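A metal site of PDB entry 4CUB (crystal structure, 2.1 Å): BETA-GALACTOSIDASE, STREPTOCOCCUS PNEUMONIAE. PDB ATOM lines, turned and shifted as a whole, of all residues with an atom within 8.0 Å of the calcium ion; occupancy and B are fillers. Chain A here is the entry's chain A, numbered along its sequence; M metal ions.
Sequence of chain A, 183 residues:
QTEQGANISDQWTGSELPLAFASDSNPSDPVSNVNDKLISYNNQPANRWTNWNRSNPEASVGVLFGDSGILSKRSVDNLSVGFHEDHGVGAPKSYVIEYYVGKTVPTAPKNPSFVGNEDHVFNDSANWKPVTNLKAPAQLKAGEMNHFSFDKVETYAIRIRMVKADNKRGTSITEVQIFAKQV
The backbone carbonyl oxygen (O) of Leu 38 is bound to the calcium ion, at 2.2 Å. The calcium ion is bound by O of Asn 33 (2.2 Å). O of Thr 174 binds the calcium ion, 2.3 Å away. The calcium ion is bound by OE1 of Glu 175, at 2.3 Å. The calcium ion is bound by OD1 of Asn 47, 2.4 Å away. The side-chain carboxylate (OD1) of Asp 36 binds the calcium ion (2.5 Å). The calcium ion has six donor atoms within binding distance.
Six residues have an atom within 4 Å of the calcium ion: Asn 33, Asp 36, Leu 38, Asn 47, Thr 174 and Glu 175. The nearest printed residue that does not touch the calcium ion is Val 34 (4.2 Å).
O of Arg 48 sits at hydrogen-bond distance from ND2 of Asn 33, at 3.1 Å. OG1 of Thr 174 is in hydrogen-bond range of N of Ser 40. O of Gly 82 sits at hydrogen-bond distance from N of Thr 174, 3.0 Å away. The side-chain carboxylate (OE2) of Glu 175 lies within hydrogen-bond range of the backbone NH (N) of Lys 37, 2.9 Å away. O of Glu 175 is in hydrogen-bond range of N of Gly 82, at 2.9 Å.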
ATOM      1  N   GLN A  11       4.115  31.349  20.435  1.00  0.00           N
ATOM      2  CA  GLN A  11       4.747  32.640  20.139  1.00  0.00           C
ATOM      3  C   GLN A  11       4.009  33.289  18.994  1.00  0.00           C
ATOM      4  O   GLN A  11       3.581  32.596  18.088  1.00  0.00           O
ATOM      5  CB  GLN A  11       6.202  32.460  19.658  1.00  0.00           C
ATOM      6  CG  GLN A  11       7.242  32.214  20.725  1.00  0.00           C
ATOM      7  CD  GLN A  11       8.599  31.904  20.105  1.00  0.00           C
ATOM      8  OE1 GLN A  11       9.015  32.567  19.165  1.00  0.00           O
ATOM      9  NE2 GLN A  11       9.291  30.884  20.611  1.00  0.00           N
ATOM     10  N   PRO A  30      17.548  26.808  24.327  1.00  0.00           N
ATOM     11  CA  PRO A  30      16.800  27.881  25.000  1.00  0.00           C
ATOM     12  C   PRO A  30      15.293  27.551  25.151  1.00  0.00           C
ATOM     13  O   PRO A  30      14.742  26.826  24.312  1.00  0.00           O
ATOM     14  CB  PRO A  30      16.982  29.068  24.052  1.00  0.00           C
ATOM     15  CG  PRO A  30      17.247  28.464  22.696  1.00  0.00           C
ATOM     16  CD  PRO A  30      17.980  27.175  22.958  1.00  0.00           C
ATOM     17  N   VAL A  31      14.644  28.080  26.184  1.00  0.00           N
ATOM     18  CA  VAL A  31      13.233  27.718  26.473  1.00  0.00           C
ATOM     19  C   VAL A  31      12.246  28.269  25.422  1.00  0.00           C
ATOM     20  O   VAL A  31      11.136  27.809  25.329  1.00  0.00           O
ATOM     21  CB  VAL A  31      12.807  28.118  27.913  1.00  0.00           C
ATOM     22  CG1 VAL A  31      12.633  29.632  28.068  1.00  0.00           C
ATOM     23  CG2 VAL A  31      11.537  27.363  28.326  1.00  0.00           C
ATOM     24  N   SER A  32      12.668  29.254  24.632  1.00  0.00           N
ATOM     25  CA  SER A  32      11.865  29.754  23.492  1.00  0.00           C
ATOM     26  C   SER A  32      11.565  28.669  22.440  1.00  0.00           C
ATOM     27  O   SER A  32      10.636  28.819  21.659  1.00  0.00           O
ATOM     28  CB  SER A  32      12.583  30.913  22.833  1.00  0.00           C
ATOM     29  OG  SER A  32      13.919  30.524  22.492  1.00  0.00           O
ATOM     30  N   ASN A  33      12.380  27.605  22.410  1.00  0.00           N
ATOM     31  CA  ASN A  33      12.089  26.400  21.598  1.00  0.00           C
ATOM     32  C   ASN A  33      10.762  25.666  21.886  1.00  0.00           C
ATOM     33  O   ASN A  33      10.190  25.122  20.957  1.00  0.00           O
ATOM     34  CB  ASN A  33      13.254  25.408  21.654  1.00  0.00           C
ATOM     35  CG  ASN A  33      14.477  25.845  20.843  1.00  0.00           C
ATOM     36  OD1 ASN A  33      14.381  26.581  19.858  1.00  0.00           O
ATOM     37  ND2 ASN A  33      15.626  25.369  21.250  1.00  0.00           N
ATOM     38  N   VAL A  34      10.276  25.667  23.135  1.00  0.00           N
ATOM     39  CA  VAL A  34       9.029  24.986  23.532  1.00  0.00           C
ATOM     40  C   VAL A  34       7.695  25.606  23.051  1.00  0.00           C
ATOM     41  O   VAL A  34       6.661  24.963  23.165  1.00  0.00           O
ATOM     42  CB  VAL A  34       8.922  24.682  25.069  1.00  0.00           C
ATOM     43  CG1 VAL A  34      10.194  24.028  25.608  1.00  0.00           C
ATOM     44  CG2 VAL A  34       8.531  25.916  25.892  1.00  0.00           C
ATOM     45  N   ASN A  35       7.706  26.839  22.541  1.00  0.00           N
ATOM     46  CA  ASN A  35       6.486  27.423  21.989  1.00  0.00           C
ATOM     47  C   ASN A  35       6.648  28.041  20.589  1.00  0.00           C
ATOM     48  O   ASN A  35       5.914  28.970  20.214  1.00  0.00           O
ATOM     49  CB  ASN A  35       5.801  28.408  22.961  1.00  0.00           C
ATOM     50  CG  ASN A  35       6.594  29.693  23.213  1.00  0.00           C
ATOM     51  OD1 ASN A  35       7.803  29.776  22.972  1.00  0.00           O
ATOM     52  ND2 ASN A  35       5.902  30.717  23.682  1.00  0.00           N
ATOM     53  N   ASP A  36       7.595  27.517  19.814  1.00  0.00           N
ATOM     54  CA  ASP A  36       7.856  28.064  18.498  1.00  0.00           C
ATOM     55  C   ASP A  36       7.118  27.317  17.381  1.00  0.00           C
ATOM     56  O   ASP A  36       7.369  27.576  16.199  1.00  0.00           O
ATOM     57  CB  ASP A  36       9.368  28.085  18.256  1.00  0.00           C
ATOM     58  CG  ASP A  36       9.988  26.674  18.198  1.00  0.00           C
ATOM     59  OD1 ASP A  36       9.284  25.619  18.219  1.00  0.00           O
ATOM     60  OD2 ASP A  36      11.220  26.622  18.141  1.00  0.00           O
ATOM     61  N   LYS A  37       6.204  26.419  17.752  1.00  0.00           N
ATOM     62  CA  LYS A  37       5.451  25.604  16.758  1.00  0.00           C
ATOM     63  C   LYS A  37       6.288  24.624  15.937  1.00  0.00           C
ATOM     64  O   LYS A  37       5.772  24.060  14.985  1.00  0.00           O
ATOM     65  CB  LYS A  37       4.596  26.487  15.821  1.00  0.00           C
ATOM     66  CG  LYS A  37       3.522  27.309  16.529  1.00  0.00           C
ATOM     67  CD  LYS A  37       3.160  28.581  15.770  1.00  0.00           C
ATOM     68  CE  LYS A  37       4.243  29.617  15.989  1.00  0.00           C
ATOM     69  NZ  LYS A  37       4.055  30.813  15.109  1.00  0.00           N
ATOM     70  N   LEU A  38       7.550  24.417  16.285  1.00  0.00           N
ATOM     71  CA  LEU A  38       8.302  23.299  15.731  1.00  0.00           C
ATOM     72  C   LEU A  38       8.307  22.141  16.726  1.00  0.00           C
ATOM     73  O   LEU A  38       8.576  22.341  17.937  1.00  0.00           O
ATOM     74  CB  LEU A  38       9.744  23.702  15.357  1.00  0.00           C
ATOM     75  CG  LEU A  38      10.028  24.892  14.428  1.00  0.00           C
ATOM     76  CD1 LEU A  38      11.501  24.915  13.995  1.00  0.00           C
ATOM     77  CD2 LEU A  38       9.147  24.979  13.189  1.00  0.00           C
ATOM     78  N   ILE A  39       8.012  20.945  16.219  1.00  0.00           N
ATOM     79  CA  ILE A  39       7.987  19.743  17.039  1.00  0.00           C
ATOM     80  C   ILE A  39       8.971  18.749  16.410  1.00  0.00           C
ATOM     81  O   ILE A  39       8.792  18.318  15.263  1.00  0.00           O
ATOM     82  CB  ILE A  39       6.554  19.153  17.180  1.00  0.00           C
ATOM     83  CG1 ILE A  39       5.621  20.177  17.836  1.00  0.00           C
ATOM     84  CG2 ILE A  39       6.575  17.895  18.030  1.00  0.00           C
ATOM     85  CD1 ILE A  39       4.181  19.748  18.038  1.00  0.00           C
ATOM     86  N   SER A  40      10.034  18.416  17.152  1.00  0.00           N
ATOM     87  CA  SER A  40      11.046  17.463  16.689  1.00  0.00           C
ATOM     88  C   SER A  40      11.468  16.520  17.803  1.00  0.00           C
ATOM     89  O   SER A  40      11.847  16.964  18.886  1.00  0.00           O
ATOM     90  CB  SER A  40      12.270  18.189  16.122  1.00  0.00           C
ATOM     91  OG  SER A  40      13.185  17.242  15.543  1.00  0.00           O
ATOM     92  N   ALA A  46      17.287  19.502  15.499  1.00  0.00           N
ATOM     93  CA  ALA A  46      17.227  19.510  16.948  1.00  0.00           C
ATOM     94  C   ALA A  46      16.458  20.768  17.360  1.00  0.00           C
ATOM     95  O   ALA A  46      16.782  21.891  16.956  1.00  0.00           O
ATOM     96  CB  ALA A  46      18.638  19.506  17.524  1.00  0.00           C
ATOM     97  N   ASN A  47      15.400  20.563  18.132  1.00  0.00           N
ATOM     98  CA  ASN A  47      14.536  21.645  18.581  1.00  0.00           C
ATOM     99  C   ASN A  47      13.950  21.280  19.912  1.00  0.00           C
ATOM    100  O   ASN A  47      13.063  20.436  19.989  1.00  0.00           O
ATOM    101  CB  ASN A  47      13.403  21.910  17.584  1.00  0.00           C
ATOM    102  CG  ASN A  47      12.516  23.041  18.033  1.00  0.00           C
ATOM    103  OD1 ASN A  47      11.478  22.820  18.657  1.00  0.00           O
ATOM    104  ND2 ASN A  47      12.941  24.275  17.775  1.00  0.00           N
ATOM    105  N   ARG A  48      14.439  21.909  20.972  1.00  0.00           N
ATOM    106  CA  ARG A  48      14.062  21.475  22.338  1.00  0.00           C
ATOM    107  C   ARG A  48      14.603  22.373  23.405  1.00  0.00           C
ATOM    108  O   ARG A  48      15.620  23.033  23.222  1.00  0.00           O
ATOM    109  CB  ARG A  48      14.501  20.020  22.588  1.00  0.00           C
ATOM    110  CG  ARG A  48      16.000  19.737  22.499  1.00  0.00           C
ATOM    111  CD  ARG A  48      16.295  18.242  22.646  1.00  0.00           C
ATOM    112  NE  ARG A  48      17.699  17.901  22.408  1.00  0.00           N
ATOM    113  CZ  ARG A  48      18.187  17.525  21.222  1.00  0.00           C
ATOM    114  NH1 ARG A  48      17.393  17.457  20.141  1.00  0.00           N
ATOM    115  NH2 ARG A  48      19.487  17.254  21.117  1.00  0.00           N
ATOM    116  N   TRP A  49      13.881  22.456  24.521  1.00  0.00           N
ATOM    117  CA  TRP A  49      14.440  22.964  25.753  1.00  0.00           C
ATOM    118  C   TRP A  49      14.988  21.757  26.477  1.00  0.00           C
ATOM    119  O   TRP A  49      14.342  20.698  26.456  1.00  0.00           O
ATOM    120  CB  TRP A  49      13.371  23.640  26.656  1.00  0.00           C
ATOM    121  CG  TRP A  49      13.919  23.878  28.048  1.00  0.00           C
ATOM    122  CD1 TRP A  49      14.628  24.972  28.476  1.00  0.00           C
ATOM    123  CD2 TRP A  49      13.822  22.997  29.182  1.00  0.00           C
ATOM    124  NE1 TRP A  49      14.959  24.828  29.805  1.00  0.00           N
ATOM    125  CE2 TRP A  49      14.479  23.621  30.264  1.00  0.00           C
ATOM    126  CE3 TRP A  49      13.228  21.735  29.385  1.00  0.00           C
ATOM    127  CZ2 TRP A  49      14.579  23.029  31.540  1.00  0.00           C
ATOM    128  CZ3 TRP A  49      13.308  21.151  30.665  1.00  0.00           C
ATOM    129  CH2 TRP A  49      13.987  21.791  31.721  1.00  0.00           C
ATOM    130  N   GLY A  82       5.240  17.723  24.872  1.00  0.00           N
ATOM    131  CA  GLY A  82       5.937  16.702  24.070  1.00  0.00           C
ATOM    132  C   GLY A  82       7.359  16.487  24.559  1.00  0.00           C
ATOM    133  O   GLY A  82       8.243  17.267  24.236  1.00  0.00           O
ATOM    134  N   ILE A 173      12.120  18.882  26.478  1.00  0.00           N
ATOM    135  CA  ILE A 173      10.783  19.183  25.914  1.00  0.00           C
ATOM    136  C   ILE A 173      10.923  19.854  24.521  1.00  0.00           C
ATOM    137  O   ILE A 173      11.550  20.895  24.375  1.00  0.00           O
ATOM    138  CB  ILE A 173       9.956  20.138  26.845  1.00  0.00           C
ATOM    139  CG1 ILE A 173       9.648  19.474  28.190  1.00  0.00           C
ATOM    140  CG2 ILE A 173       8.654  20.588  26.195  1.00  0.00           C
ATOM    141  CD1 ILE A 173       9.133  20.444  29.245  1.00  0.00           C
ATOM    142  N   THR A 174      10.328  19.261  23.496  1.00  0.00           N
ATOM    143  CA  THR A 174      10.363  19.921  22.190  1.00  0.00           C
ATOM    144  C   THR A 174       9.303  21.036  22.001  1.00  0.00           C
ATOM    145  O   THR A 174       9.550  22.037  21.288  1.00  0.00           O
ATOM    146  CB  THR A 174      10.349  18.892  21.027  1.00  0.00           C
ATOM    147  OG1 THR A 174      10.385  19.621  19.795  1.00  0.00           O
ATOM    148  CG2 THR A 174       9.087  18.022  21.041  1.00  0.00           C
ATOM    149  N   GLU A 175       8.153  20.889  22.679  1.00  0.00           N
ATOM    150  CA  GLU A 175       7.018  21.807  22.518  1.00  0.00           C
ATOM    151  C   GLU A 175       5.992  21.611  23.639  1.00  0.00           C
ATOM    152  O   GLU A 175       5.733  20.489  24.042  1.00  0.00           O
ATOM    153  CB  GLU A 175       6.324  21.554  21.160  1.00  0.00           C
ATOM    154  CG  GLU A 175       5.316  22.595  20.699  1.00  0.00           C
ATOM    155  CD  GLU A 175       5.959  23.903  20.290  1.00  0.00           C
ATOM    156  OE1 GLU A 175       7.195  23.991  20.265  1.00  0.00           O
ATOM    157  OE2 GLU A 175       5.224  24.872  20.035  1.00  0.00           O
ATOM    158  N   VAL A 176       5.416  22.700  24.143  1.00  0.00           N
ATOM    159  CA  VAL A 176       4.189  22.612  24.938  1.00  0.00           C
ATOM    160  C   VAL A 176       3.056  23.301  24.176  1.00  0.00           C
ATOM    161  O   VAL A 176       3.311  24.090  23.252  1.00  0.00           O
ATOM    162  CB  VAL A 176       4.327  23.268  26.324  1.00  0.00           C
ATOM    163  CG1 VAL A 176       5.529  22.701  27.091  1.00  0.00           C
ATOM    164  CG2 VAL A 176       4.414  24.789  26.204  1.00  0.00           C
HETATM  165 CA    CA M   1       9.393  23.549  19.564  1.00  0.00          CA
